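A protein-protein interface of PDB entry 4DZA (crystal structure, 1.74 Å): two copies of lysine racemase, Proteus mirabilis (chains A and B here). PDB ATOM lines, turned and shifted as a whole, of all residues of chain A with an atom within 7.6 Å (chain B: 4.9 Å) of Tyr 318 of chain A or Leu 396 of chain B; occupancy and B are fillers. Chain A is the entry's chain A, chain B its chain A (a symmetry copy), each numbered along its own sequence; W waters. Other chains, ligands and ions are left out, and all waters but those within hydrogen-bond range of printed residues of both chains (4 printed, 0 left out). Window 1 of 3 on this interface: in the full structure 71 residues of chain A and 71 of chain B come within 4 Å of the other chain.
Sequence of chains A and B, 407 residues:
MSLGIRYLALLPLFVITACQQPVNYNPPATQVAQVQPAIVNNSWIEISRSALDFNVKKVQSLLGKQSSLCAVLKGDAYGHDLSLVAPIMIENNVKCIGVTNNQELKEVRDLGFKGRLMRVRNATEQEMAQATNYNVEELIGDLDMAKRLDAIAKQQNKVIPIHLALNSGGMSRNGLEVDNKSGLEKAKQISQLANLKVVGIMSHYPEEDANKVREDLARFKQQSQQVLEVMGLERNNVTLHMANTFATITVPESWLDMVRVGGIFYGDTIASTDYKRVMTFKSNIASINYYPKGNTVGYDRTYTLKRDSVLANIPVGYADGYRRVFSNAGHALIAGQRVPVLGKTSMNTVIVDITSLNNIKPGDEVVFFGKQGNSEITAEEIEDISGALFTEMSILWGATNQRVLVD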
ATOM      1  N   TYR A 299       7.729 -14.015  -1.789  1.00  0.00           N
ATOM      2  CA  TYR A 299       6.998 -12.927  -1.065  1.00  0.00           C
ATOM      3  C   TYR A 299       5.989 -12.196  -1.988  1.00  0.00           C
ATOM      4  O   TYR A 299       6.264 -11.990  -3.180  1.00  0.00           O
ATOM      5  CB  TYR A 299       7.958 -11.889  -0.446  1.00  0.00           C
ATOM      6  CG  TYR A 299       8.693 -12.366   0.807  1.00  0.00           C
ATOM      7  CD1 TYR A 299       8.017 -12.507   2.017  1.00  0.00           C
ATOM      8  CD2 TYR A 299      10.079 -12.610   0.786  1.00  0.00           C
ATOM      9  CE1 TYR A 299       8.681 -12.898   3.177  1.00  0.00           C
ATOM     10  CE2 TYR A 299      10.734 -13.056   1.912  1.00  0.00           C
ATOM     11  CZ  TYR A 299      10.065 -13.151   3.117  1.00  0.00           C
ATOM     12  OH  TYR A 299      10.733 -13.580   4.263  1.00  0.00           O
ATOM     13  N   VAL A 316      21.221 -18.424  -2.750  1.00  0.00           N
ATOM     14  CA  VAL A 316      21.727 -17.117  -3.042  1.00  0.00           C
ATOM     15  C   VAL A 316      20.528 -16.165  -2.997  1.00  0.00           C
ATOM     16  O   VAL A 316      19.435 -16.517  -3.500  1.00  0.00           O
ATOM     17  CB  VAL A 316      22.316 -17.139  -4.507  1.00  0.00           C
ATOM     18  CG1 VAL A 316      22.489 -15.709  -5.043  1.00  0.00           C
ATOM     19  CG2 VAL A 316      23.664 -17.853  -4.463  1.00  0.00           C
ATOM     20  N   GLY A 317      20.707 -15.005  -2.347  1.00  0.00           N
ATOM     21  CA  GLY A 317      19.637 -13.988  -2.277  1.00  0.00           C
ATOM     22  C   GLY A 317      20.214 -12.593  -2.268  1.00  0.00           C
ATOM     23  O   GLY A 317      21.421 -12.364  -2.588  1.00  0.00           O
ATOM     24  N   TYR A 318      19.425 -11.628  -1.846  1.00  0.00           N
ATOM     25  CA  TYR A 318      19.940 -10.267  -1.850  1.00  0.00           C
ATOM     26  C   TYR A 318      21.069  -9.945  -0.844  1.00  0.00           C
ATOM     27  O   TYR A 318      21.834  -9.037  -1.047  1.00  0.00           O
ATOM     28  CB  TYR A 318      18.816  -9.186  -1.828  1.00  0.00           C
ATOM     29  CG  TYR A 318      17.910  -9.150  -0.586  1.00  0.00           C
ATOM     30  CD1 TYR A 318      18.310  -8.510   0.583  1.00  0.00           C
ATOM     31  CD2 TYR A 318      16.625  -9.668  -0.651  1.00  0.00           C
ATOM     32  CE1 TYR A 318      17.435  -8.445   1.676  1.00  0.00           C
ATOM     33  CE2 TYR A 318      15.763  -9.609   0.401  1.00  0.00           C
ATOM     34  CZ  TYR A 318      16.181  -9.027   1.568  1.00  0.00           C
ATOM     35  OH  TYR A 318      15.284  -8.918   2.598  1.00  0.00           O
ATOM     36  N   ALA A 319      21.228 -10.776   0.164  1.00  0.00           N
ATOM     37  CA  ALA A 319      22.366 -10.657   1.084  1.00  0.00           C
ATOM     38  C   ALA A 319      23.650 -11.098   0.405  1.00  0.00           C
ATOM     39  O   ALA A 319      24.767 -10.873   0.919  1.00  0.00           O
ATOM     40  CB  ALA A 319      22.144 -11.457   2.276  1.00  0.00           C
ATOM     41  N   ASP A 320      23.480 -11.804  -0.711  1.00  0.00           N
ATOM     42  CA  ASP A 320      24.642 -12.140  -1.549  1.00  0.00           C
ATOM     43  C   ASP A 320      24.697 -11.162  -2.743  1.00  0.00           C
ATOM     44  O   ASP A 320      25.450 -11.421  -3.751  1.00  0.00           O
ATOM     45  CB  ASP A 320      24.475 -13.556  -2.079  1.00  0.00           C
ATOM     46  CG  ASP A 320      24.276 -14.570  -0.981  1.00  0.00           C
ATOM     47  OD1 ASP A 320      25.247 -14.815  -0.262  1.00  0.00           O
ATOM     48  OD2 ASP A 320      23.140 -15.096  -0.777  1.00  0.00           O
ATOM     49  N   GLY A 321      24.022 -10.022  -2.618  1.00  0.00           N
ATOM     50  CA  GLY A 321      24.021  -9.006  -3.686  1.00  0.00           C
ATOM     51  C   GLY A 321      23.186  -9.380  -4.873  1.00  0.00           C
ATOM     52  O   GLY A 321      23.237  -8.687  -5.906  1.00  0.00           O
ATOM     53  N   TYR A 322      22.461 -10.486  -4.757  1.00  0.00           N
ATOM     54  CA  TYR A 322      21.521 -10.893  -5.827  1.00  0.00           C
ATOM     55  C   TYR A 322      20.183 -10.168  -5.628  1.00  0.00           C
ATOM     56  O   TYR A 322      19.221 -10.712  -5.133  1.00  0.00           O
ATOM     57  CB  TYR A 322      21.376 -12.407  -5.972  1.00  0.00           C
ATOM     58  CG  TYR A 322      20.978 -12.777  -7.404  1.00  0.00           C
ATOM     59  CD1 TYR A 322      19.708 -13.232  -7.674  1.00  0.00           C
ATOM     60  CD2 TYR A 322      21.896 -12.642  -8.464  1.00  0.00           C
ATOM     61  CE1 TYR A 322      19.337 -13.595  -8.960  1.00  0.00           C
ATOM     62  CE2 TYR A 322      21.497 -12.926  -9.767  1.00  0.00           C
ATOM     63  CZ  TYR A 322      20.219 -13.414  -9.985  1.00  0.00           C
ATOM     64  OH  TYR A 322      19.775 -13.719 -11.250  1.00  0.00           O
ATOM     65  N   ARG A 323      20.220  -8.875  -5.926  1.00  0.00           N
ATOM     66  CA  ARG A 323      19.265  -7.928  -5.390  1.00  0.00           C
ATOM     67  C   ARG A 323      17.853  -8.124  -5.914  1.00  0.00           C
ATOM     68  O   ARG A 323      17.633  -8.887  -6.844  1.00  0.00           O
ATOM     69  CB  ARG A 323      19.713  -6.496  -5.695  1.00  0.00           C
ATOM     70  CG  ARG A 323      21.057  -6.032  -4.993  1.00  0.00           C
ATOM     71  CD  ARG A 323      21.086  -4.477  -4.869  1.00  0.00           C
ATOM     72  NE  ARG A 323      20.714  -3.770  -6.111  1.00  0.00           N
ATOM     73  CZ  ARG A 323      21.564  -3.503  -7.099  1.00  0.00           C
ATOM     74  NH1 ARG A 323      22.801  -3.946  -7.026  1.00  0.00           N
ATOM     75  NH2 ARG A 323      21.166  -2.776  -8.183  1.00  0.00           N
ATOM     76  N   ARG A 324      16.914  -7.373  -5.308  1.00  0.00           N
ATOM     77  CA  ARG A 324      15.494  -7.445  -5.631  1.00  0.00           C
ATOM     78  C   ARG A 324      15.237  -7.025  -7.061  1.00  0.00           C
ATOM     79  O   ARG A 324      14.199  -7.343  -7.655  1.00  0.00           O
ATOM     80  CB  ARG A 324      14.744  -6.513  -4.699  1.00  0.00           C
ATOM     81  CG  ARG A 324      14.431  -7.158  -3.359  1.00  0.00           C
ATOM     82  CD  ARG A 324      13.129  -7.997  -3.502  1.00  0.00           C
ATOM     83  NE  ARG A 324      12.889  -9.009  -2.487  1.00  0.00           N
ATOM     84  CZ  ARG A 324      12.035  -8.864  -1.456  1.00  0.00           C
ATOM     85  NH1 ARG A 324      11.396  -7.714  -1.274  1.00  0.00           N
ATOM     86  NH2 ARG A 324      11.832  -9.863  -0.596  1.00  0.00           N
ATOM     87  N   VAL A 325      16.190  -6.299  -7.601  1.00  0.00           N
ATOM     88  CA  VAL A 325      16.217  -5.965  -9.020  1.00  0.00           C
ATOM     89  C   VAL A 325      16.107  -7.255  -9.926  1.00  0.00           C
ATOM     90  O   VAL A 325      15.573  -7.212 -11.066  1.00  0.00           O
ATOM     91  CB  VAL A 325      17.488  -5.142  -9.215  1.00  0.00           C
ATOM     92  CG1 VAL A 325      18.526  -5.812  -9.953  1.00  0.00           C
ATOM     93  CG2 VAL A 325      17.261  -3.679  -9.482  1.00  0.00           C
ATOM     94  N   PHE A 326      16.519  -8.409  -9.396  1.00  0.00           N
ATOM     95  CA  PHE A 326      16.469  -9.661 -10.164  1.00  0.00           C
ATOM     96  C   PHE A 326      15.140 -10.395 -10.075  1.00  0.00           C
ATOM     97  O   PHE A 326      14.968 -11.427 -10.718  1.00  0.00           O
ATOM     98  CB  PHE A 326      17.629 -10.618  -9.786  1.00  0.00           C
ATOM     99  CG  PHE A 326      18.989 -10.127 -10.236  1.00  0.00           C
ATOM    100  CD1 PHE A 326      19.438 -10.398 -11.527  1.00  0.00           C
ATOM    101  CD2 PHE A 326      19.846  -9.461  -9.349  1.00  0.00           C
ATOM    102  CE1 PHE A 326      20.727  -9.976 -11.954  1.00  0.00           C
ATOM    103  CE2 PHE A 326      21.130  -8.997  -9.771  1.00  0.00           C
ATOM    104  CZ  PHE A 326      21.552  -9.241 -11.090  1.00  0.00           C
ATOM    105  N   SER A 327      14.202  -9.859  -9.270  1.00  0.00           N
ATOM    106  CA  SER A 327      12.913 -10.487  -9.006  1.00  0.00           C
ATOM    107  C   SER A 327      12.129 -10.638 -10.324  1.00  0.00           C
ATOM    108  O   SER A 327      11.956  -9.647 -11.024  1.00  0.00           O
ATOM    109  CB  SER A 327      12.118  -9.638  -8.040  1.00  0.00           C
ATOM    110  OG  SER A 327      12.774  -9.521  -6.737  1.00  0.00           O
ATOM    111  N   LYS A 344      10.031 -12.898  -6.127  1.00  0.00           N
ATOM    112  CA  LYS A 344      10.918 -11.901  -5.533  1.00  0.00           C
ATOM    113  C   LYS A 344      12.090 -12.676  -4.983  1.00  0.00           C
ATOM    114  O   LYS A 344      11.886 -13.781  -4.439  1.00  0.00           O
ATOM    115  CB  LYS A 344      10.208 -11.151  -4.390  1.00  0.00           C
ATOM    116  CG  LYS A 344       9.260 -10.083  -4.868  1.00  0.00           C
ATOM    117  CD  LYS A 344       8.678  -9.298  -3.715  1.00  0.00           C
ATOM    118  CE  LYS A 344       7.792  -8.170  -4.221  1.00  0.00           C
ATOM    119  NZ  LYS A 344       7.336  -7.288  -3.070  1.00  0.00           N
ATOM    120  N   THR A 345      13.295 -12.097  -5.105  1.00  0.00           N
ATOM    121  CA  THR A 345      14.451 -12.682  -4.447  1.00  0.00           C
ATOM    122  C   THR A 345      14.201 -12.649  -2.935  1.00  0.00           C
ATOM    123  O   THR A 345      13.569 -11.736  -2.435  1.00  0.00           O
ATOM    124  CB  THR A 345      15.775 -11.982  -4.856  1.00  0.00           C
ATOM    125  OG1 THR A 345      15.764 -10.591  -4.498  1.00  0.00           O
ATOM    126  CG2 THR A 345      16.001 -12.085  -6.380  1.00  0.00           C
ATOM    127  N   SER A 346      14.642 -13.664  -2.216  1.00  0.00           N
ATOM    128  CA  SER A 346      14.576 -13.579  -0.748  1.00  0.00           C
ATOM    129  C   SER A 346      15.930 -13.125  -0.240  1.00  0.00           C
ATOM    130  O   SER A 346      16.867 -13.022  -1.024  1.00  0.00           O
ATOM    131  CB  SER A 346      14.243 -14.936  -0.151  1.00  0.00           C
ATOM    132  OG  SER A 346      12.913 -15.317  -0.456  1.00  0.00           O
ATOM    133  N   MET A 347      16.074 -12.925   1.069  1.00  0.00           N
ATOM    134  CA  MET A 347      17.380 -12.478   1.543  1.00  0.00           C
ATOM    135  C   MET A 347      18.463 -13.512   1.176  1.00  0.00           C
ATOM    136  O   MET A 347      19.586 -13.089   0.951  1.00  0.00           O
ATOM    137  CB  MET A 347      17.347 -12.281   3.064  1.00  0.00           C
ATOM    138  CG  MET A 347      18.608 -11.689   3.594  1.00  0.00           C
ATOM    139  SD  MET A 347      18.368 -11.290   5.407  1.00  0.00           S
ATOM    140  CE  MET A 347      16.973 -10.169   5.323  1.00  0.00           C
ATOM    141  N   ASN A 348      18.190 -14.808   1.360  1.00  0.00           N
ATOM    142  CA  ASN A 348      19.226 -15.785   1.249  1.00  0.00           C
ATOM    143  C   ASN A 348      18.964 -16.913   0.250  1.00  0.00           C
ATOM    144  O   ASN A 348      19.750 -17.876   0.183  1.00  0.00           O
ATOM    145  CB  ASN A 348      19.504 -16.376   2.637  1.00  0.00           C
ATOM    146  CG  ASN A 348      20.007 -15.346   3.592  1.00  0.00           C
ATOM    147  OD1 ASN A 348      19.278 -14.881   4.485  1.00  0.00           O
ATOM    148  ND2 ASN A 348      21.200 -14.874   3.335  1.00  0.00           N
ATOM    149  N   THR A 349      17.866 -16.810  -0.527  1.00  0.00           N
ATOM    150  CA  THR A 349      17.367 -17.927  -1.364  1.00  0.00           C
ATOM    151  C   THR A 349      16.701 -17.340  -2.576  1.00  0.00           C
ATOM    152  O   THR A 349      16.023 -16.282  -2.480  1.00  0.00           O
ATOM    153  CB  THR A 349      16.314 -18.832  -0.592  1.00  0.00           C
ATOM    154  OG1 THR A 349      16.937 -19.427   0.584  1.00  0.00           O
ATOM    155  CG2 THR A 349      15.771 -19.962  -1.438  1.00  0.00           C
ATOM    156  N   VAL A 350      17.011 -17.948  -3.702  1.00  0.00           N
ATOM    157  CA  VAL A 350      16.326 -17.673  -4.965  1.00  0.00           C
ATOM    158  C   VAL A 350      15.708 -19.012  -5.507  1.00  0.00           C
ATOM    159  O   VAL A 350      16.273 -20.092  -5.361  1.00  0.00           O
ATOM    160  CB  VAL A 350      17.231 -16.928  -5.950  1.00  0.00           C
ATOM    161  CG1 VAL A 350      18.417 -17.757  -6.334  1.00  0.00           C
ATOM    162  CG2 VAL A 350      16.421 -16.454  -7.179  1.00  0.00           C
ATOM    163  N   LEU A 396      29.674  -5.149  -5.546  1.00  0.00           N
ATOM    164  CA  LEU A 396      28.719  -5.613  -4.517  1.00  0.00           C
ATOM    165  C   LEU A 396      28.604  -7.135  -4.370  1.00  0.00           C
ATOM    166  O   LEU A 396      28.586  -7.628  -3.272  1.00  0.00           O
ATOM    167  CB  LEU A 396      27.318  -4.982  -4.713  1.00  0.00           C
ATOM    168  CG  LEU A 396      27.359  -3.478  -4.631  1.00  0.00           C
ATOM    169  CD1 LEU A 396      25.967  -2.855  -4.873  1.00  0.00           C
ATOM    170  CD2 LEU A 396      27.900  -3.024  -3.293  1.00  0.00           C
ATOM    171  N   TRP A 397      28.712  -7.868  -5.473  1.00  0.00           N
ATOM    172  CA  TRP A 397      28.907  -9.318  -5.385  1.00  0.00           C
ATOM    173  C   TRP A 397      30.200  -9.677  -4.638  1.00  0.00           C
ATOM    174  O   TRP A 397      30.213 -10.615  -3.880  1.00  0.00           O
ATOM    175  CB  TRP A 397      28.906  -9.955  -6.803  1.00  0.00           C
ATOM    176  CG  TRP A 397      27.539 -10.033  -7.422  1.00  0.00           C
ATOM    177  CD1 TRP A 397      26.295  -9.832  -6.824  1.00  0.00           C
ATOM    178  CD2 TRP A 397      27.287 -10.316  -8.775  1.00  0.00           C
ATOM    179  NE1 TRP A 397      25.287 -10.052  -7.746  1.00  0.00           N
ATOM    180  CE2 TRP A 397      25.885 -10.263  -8.976  1.00  0.00           C
ATOM    181  CE3 TRP A 397      28.127 -10.479  -9.878  1.00  0.00           C
ATOM    182  CZ2 TRP A 397      25.286 -10.520 -10.230  1.00  0.00           C
ATOM    183  CZ3 TRP A 397      27.528 -10.699 -11.149  1.00  0.00           C
ATOM    184  CH2 TRP A 397      26.134 -10.754 -11.298  1.00  0.00           C
ATOM    185  N   ALA A 399      31.776  -8.036  -2.428  1.00  0.00           N
ATOM    186  CA  ALA A 399      31.647  -7.721  -0.977  1.00  0.00           C
ATOM    187  C   ALA A 399      30.817  -8.713  -0.162  1.00  0.00           C
ATOM    188  O   ALA A 399      30.925  -8.746   1.094  1.00  0.00           O
ATOM    189  CB  ALA A 399      31.102  -6.303  -0.816  1.00  0.00           C
ATOM    190  N   THR A 400      29.976  -9.494  -0.833  1.00  0.00           N
ATOM    191  CA  THR A 400      29.042 -10.380  -0.210  1.00  0.00           C
ATOM    192  C   THR A 400      29.184 -11.895  -0.532  1.00  0.00           C
ATOM    193  O   THR A 400      28.343 -12.673  -0.153  1.00  0.00           O
ATOM    194  CB  THR A 400      27.609  -9.931  -0.498  1.00  0.00           C
ATOM    195  OG1 THR A 400      27.404  -9.954  -1.920  1.00  0.00           O
ATOM    196  CG2 THR A 400      27.359  -8.470   0.041  1.00  0.00           C
ATOM    197  N   GLY B 321      28.396   0.877  -1.108  1.00  0.00           N
ATOM    198  CA  GLY B 321      26.952   0.603  -1.211  1.00  0.00           C
ATOM    199  C   GLY B 321      26.115   1.835  -1.377  1.00  0.00           C
ATOM    200  O   GLY B 321      24.875   1.753  -1.308  1.00  0.00           O
ATOM    201  N   ARG B 323      24.833   3.512  -3.767  1.00  0.00           N
ATOM    202  CA  ARG B 323      24.739   3.104  -5.152  1.00  0.00           C
ATOM    203  C   ARG B 323      24.343   4.229  -6.093  1.00  0.00           C
ATOM    204  O   ARG B 323      23.957   5.303  -5.653  1.00  0.00           O
ATOM    205  CB  ARG B 323      23.734   1.959  -5.297  1.00  0.00           C
ATOM    206  CG  ARG B 323      24.134   0.598  -4.587  1.00  0.00           C
ATOM    207  CD  ARG B 323      23.408  -0.599  -5.276  1.00  0.00           C
ATOM    208  NE  ARG B 323      21.966  -0.374  -5.504  1.00  0.00           N
ATOM    209  CZ  ARG B 323      21.025  -0.594  -4.589  1.00  0.00           C
ATOM    210  NH1 ARG B 323      21.375  -0.967  -3.376  1.00  0.00           N
ATOM    211  NH2 ARG B 323      19.705  -0.438  -4.897  1.00  0.00           N
ATOM    212  N   LEU B 389      13.213  -2.715  -0.463  1.00  0.00           N
ATOM    213  CA  LEU B 389      13.071  -2.582   1.016  1.00  0.00           C
ATOM    214  C   LEU B 389      14.389  -2.189   1.704  1.00  0.00           C
ATOM    215  O   LEU B 389      15.505  -2.501   1.206  1.00  0.00           O
ATOM    216  CB  LEU B 389      12.546  -3.865   1.631  1.00  0.00           C
ATOM    217  CG  LEU B 389      13.534  -5.057   1.795  1.00  0.00           C
ATOM    218  CD1 LEU B 389      12.867  -6.236   2.466  1.00  0.00           C
ATOM    219  CD2 LEU B 389      14.186  -5.456   0.433  1.00  0.00           C
ATOM    220  N   THR B 391      15.894  -3.306   4.195  1.00  0.00           N
ATOM    221  CA  THR B 391      16.750  -4.370   4.738  1.00  0.00           C
ATOM    222  C   THR B 391      17.824  -4.701   3.696  1.00  0.00           C
ATOM    223  O   THR B 391      18.934  -4.980   4.049  1.00  0.00           O
ATOM    224  CB  THR B 391      15.973  -5.643   5.044  1.00  0.00           C
ATOM    225  OG1 THR B 391      14.764  -5.321   5.801  1.00  0.00           O
ATOM    226  CG2 THR B 391      16.845  -6.533   5.894  1.00  0.00           C
ATOM    227  N   GLU B 392      17.478  -4.635   2.412  1.00  0.00           N
ATOM    228  CA  GLU B 392      18.512  -4.894   1.360  1.00  0.00           C
ATOM    229  C   GLU B 392      19.626  -3.840   1.501  1.00  0.00           C
ATOM    230  O   GLU B 392      20.788  -4.169   1.383  1.00  0.00           O
ATOM    231  CB  GLU B 392      17.909  -4.863  -0.085  1.00  0.00           C
ATOM    232  CG  GLU B 392      18.940  -4.978  -1.234  1.00  0.00           C
ATOM    233  CD  GLU B 392      18.270  -5.165  -2.607  1.00  0.00           C
ATOM    234  OE1 GLU B 392      18.006  -4.133  -3.271  1.00  0.00           O
ATOM    235  OE2 GLU B 392      17.876  -6.319  -2.916  1.00  0.00           O
ATOM    236  N   MET B 393      19.255  -2.569   1.701  1.00  0.00           N
ATOM    237  CA  MET B 393      20.239  -1.485   1.876  1.00  0.00           C
ATOM    238  C   MET B 393      21.091  -1.652   3.099  1.00  0.00           C
ATOM    239  O   MET B 393      22.293  -1.459   3.027  1.00  0.00           O
ATOM    240  CB  MET B 393      19.572  -0.071   1.870  1.00  0.00           C
ATOM    241  CG  MET B 393      20.584   1.100   1.721  1.00  0.00           C
ATOM    242  SD  MET B 393      21.382   1.147   0.071  1.00  0.00           S
ATOM    243  CE  MET B 393      20.056   1.605  -1.054  1.00  0.00           C
ATOM    244  N   SER B 394      20.469  -1.892   4.250  1.00  0.00           N
ATOM    245  CA  SER B 394      21.260  -2.069   5.485  1.00  0.00           C
ATOM    246  C   SER B 394      22.266  -3.231   5.345  1.00  0.00           C
ATOM    247  O   SER B 394      23.400  -3.151   5.846  1.00  0.00           O
ATOM    248  CB  SER B 394      20.392  -2.199   6.761  1.00  0.00           C
ATOM    249  OG  SER B 394      19.558  -3.378   6.748  1.00  0.00           O
ATOM    250  N   ILE B 395      21.841  -4.289   4.669  1.00  0.00           N
ATOM    251  CA  ILE B 395      22.720  -5.489   4.465  1.00  0.00           C
ATOM    252  C   ILE B 395      23.866  -5.076   3.573  1.00  0.00           C
ATOM    253  O   ILE B 395      25.051  -5.377   3.873  1.00  0.00           O
ATOM    254  CB  ILE B 395      21.909  -6.657   3.835  1.00  0.00           C
ATOM    255  CG1 ILE B 395      20.865  -7.146   4.877  1.00  0.00           C
ATOM    256  CG2 ILE B 395      22.835  -7.775   3.380  1.00  0.00           C
ATOM    257  CD1 ILE B 395      19.957  -8.322   4.462  1.00  0.00           C
ATOM    258  N   LEU B 396      23.554  -4.412   2.476  1.00  0.00           N
ATOM    259  CA  LEU B 396      24.631  -4.011   1.546  1.00  0.00           C
ATOM    260  C   LEU B 396      25.564  -2.910   2.061  1.00  0.00           C
ATOM    261  O   LEU B 396      26.753  -3.018   1.913  1.00  0.00           O
ATOM    262  CB  LEU B 396      24.069  -3.635   0.152  1.00  0.00           C
ATOM    263  CG  LEU B 396      23.335  -4.783  -0.491  1.00  0.00           C
ATOM    264  CD1 LEU B 396      22.740  -4.384  -1.859  1.00  0.00           C
ATOM    265  CD2 LEU B 396      24.244  -5.980  -0.655  1.00  0.00           C
ATOM    266  N   TRP B 397      25.030  -1.957   2.819  1.00  0.00           N
ATOM    267  CA  TRP B 397      25.888  -1.049   3.585  1.00  0.00           C
ATOM    268  C   TRP B 397      26.764  -1.803   4.595  1.00  0.00           C
ATOM    269  O   TRP B 397      27.906  -1.459   4.773  1.00  0.00           O
ATOM    270  CB  TRP B 397      25.033   0.028   4.309  1.00  0.00           C
ATOM    271  CG  TRP B 397      24.495   1.084   3.385  1.00  0.00           C
ATOM    272  CD1 TRP B 397      24.840   1.346   2.059  1.00  0.00           C
ATOM    273  CD2 TRP B 397      23.494   2.011   3.724  1.00  0.00           C
ATOM    274  NE1 TRP B 397      24.138   2.444   1.596  1.00  0.00           N
ATOM    275  CE2 TRP B 397      23.238   2.810   2.581  1.00  0.00           C
ATOM    276  CE3 TRP B 397      22.685   2.158   4.852  1.00  0.00           C
ATOM    277  CZ2 TRP B 397      22.292   3.860   2.584  1.00  0.00           C
ATOM    278  CZ3 TRP B 397      21.705   3.189   4.844  1.00  0.00           C
ATOM    279  CH2 TRP B 397      21.552   4.039   3.738  1.00  0.00           C
ATOM    280  N   GLY B 398      26.195  -2.781   5.285  1.00  0.00           N
ATOM    281  CA  GLY B 398      26.913  -3.483   6.338  1.00  0.00           C
ATOM    282  C   GLY B 398      28.051  -4.298   5.723  1.00  0.00           C
ATOM    283  O   GLY B 398      29.113  -4.439   6.331  1.00  0.00           O
ATOM    284  N   ALA B 399      27.817  -4.795   4.514  1.00  0.00           N
ATOM    285  CA  ALA B 399      28.868  -5.583   3.810  1.00  0.00           C
ATOM    286  C   ALA B 399      30.051  -4.773   3.282  1.00  0.00           C
ATOM    287  O   ALA B 399      31.133  -5.352   2.989  1.00  0.00           O
ATOM    288  CB  ALA B 399      28.222  -6.390   2.684  1.00  0.00           C
ATOM    289  N   THR B 400      29.868  -3.466   3.123  1.00  0.00           N
ATOM    290  CA  THR B 400      30.829  -2.594   2.522  1.00  0.00           C
ATOM    291  C   THR B 400      31.373  -1.432   3.399  1.00  0.00           C
ATOM    292  O   THR B 400      32.075  -0.582   2.908  1.00  0.00           O
ATOM    293  CB  THR B 400      30.286  -2.028   1.209  1.00  0.00           C
ATOM    294  OG1 THR B 400      29.089  -1.285   1.496  1.00  0.00           O
ATOM    295  CG2 THR B 400      29.948  -3.187   0.194  1.00  0.00           C
HETATM  296  O   HOH W   1      17.753  -3.739  -5.778  1.00  0.00           O
HETATM  297  O   HOH W   2      32.442  -7.774   3.185  1.00  0.00           O
HETATM  298  O   HOH W   3      11.700  -4.701  -2.499  1.00  0.00           O
HETATM  299  O   HOH W   4      18.984  -0.862  -7.716  1.00  0.00           O
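Tyr 318 of chain A touches Leu 389 of chain B (OH to CD1, 3.6 Å).
Tyr 318 of chain A touches Leu 396 of chain B.
Arg 323 of chain A touches Leu 396 of chain B (CD to CD1, 3.4 Å).
NH1 of Arg 324 of chain A touches CD2 of Leu 389 of chain B (3.97 Å).
Met 347 of chain A touches Ile 395 of chain B.
CD1 of Leu 396 of chain A touches CD of Arg 323 of chain B (3.4 Å).
Thr 400 of chain B touches Ala 399 of chain A (CG2 to CB, 3.5 Å).
Ala 399 of chain B touches Thr 400 of chain A.
The guanidinium group of Arg 323 of chain A is in salt-bridge range of the side-chain carboxylate of Glu 392 of chain B.
N of Arg 324 of chain A is in hydrogen-bond range of OE2 of Glu 392 of chain B.
Arg 323 of chain B touches its own counterpart, Arg 323 of chain A.
Arg 323 of chain A touches Leu 396 of chain B, and with the chains exchanged Leu 396 of chain A touches Arg 323 of chain B.
Ala 399 of chain B touches its own counterpart, Ala 399 of chain A.
6 positions are printed for both chains.
Of the 16 pairs that touch across the chains among the printed residues, 6 have their exchanged pair printed and touching as well.
Hydrophobic or aromatic side chains of chain B that line the printed part of chain A: Leu 389, Ile 395, Leu 396 and Ala 399.
Of the 24 printed residues of chain A, 8 touch a printed residue of chain B.
Among the printed residues, Asp or Glu carboxylates within 4 Å of a Lys or Arg side-chain nitrogen of the other chain: Arg 323 of chain A with Glu 392 of chain B.
Water W1 bridges OE1 of Glu 392 of chain B (2.6 Å) and NE of Arg 323 of chain A (3.0 Å).
Water W2 bridges the backbone carbonyl oxygen of Ala 399 of chain A (2.8 Å) and the backbone carbonyl oxygen of Ala 399 of chain B (2.8 Å).
Water W4 lies within hydrogen-bond range of NH2 of Arg 323 of chain A (2.9 Å) and NH2 of Arg 323 of chain B (2.9 Å).
Printed residues of chain B within 4 Å of Tyr 318 of chain A: Leu 389 (3.6 Å), Glu 392 (3.2 Å), Ile 395 (3.8 Å) and Leu 396 (3.9 Å).
Of the printed residues of chain B, Arg 324 of chain A touches Leu 389 (3.97 Å) and Glu 392 (2.8 Å).
Printed residues of chain B within 4 Å of Thr 400 of chain A: Ala 399.
Of the printed residues of chain A, Arg 323 of chain B touches Arg 323 and Leu 396.
Of the printed residues of chain A, Thr 391 of chain B touches Met 347 (3.7 Å).
Of chain A, only Tyr 318 and Arg 323 come within 4 Å of Leu 396 of chain B.
The nearest residue of chain A that does not touch Leu 396 of chain B is Thr 400 of chain A (4.05 Å).
The backbone NH (N) of Ala 319 of chain A is in hydrogen-bond range of the backbone carbonyl oxygen (O) of Met 347 of chain A (2.9 Å).
The side-chain hydroxyl (OG1) of Thr 400 of chain A sits at hydrogen-bond distance from the backbone carbonyl oxygen (O) of Leu 396 of chain A (2.9 Å).
O of Trp 397 of chain B lies within hydrogen-bond range of OG1 of Thr 400 of chain B (3.5 Å).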
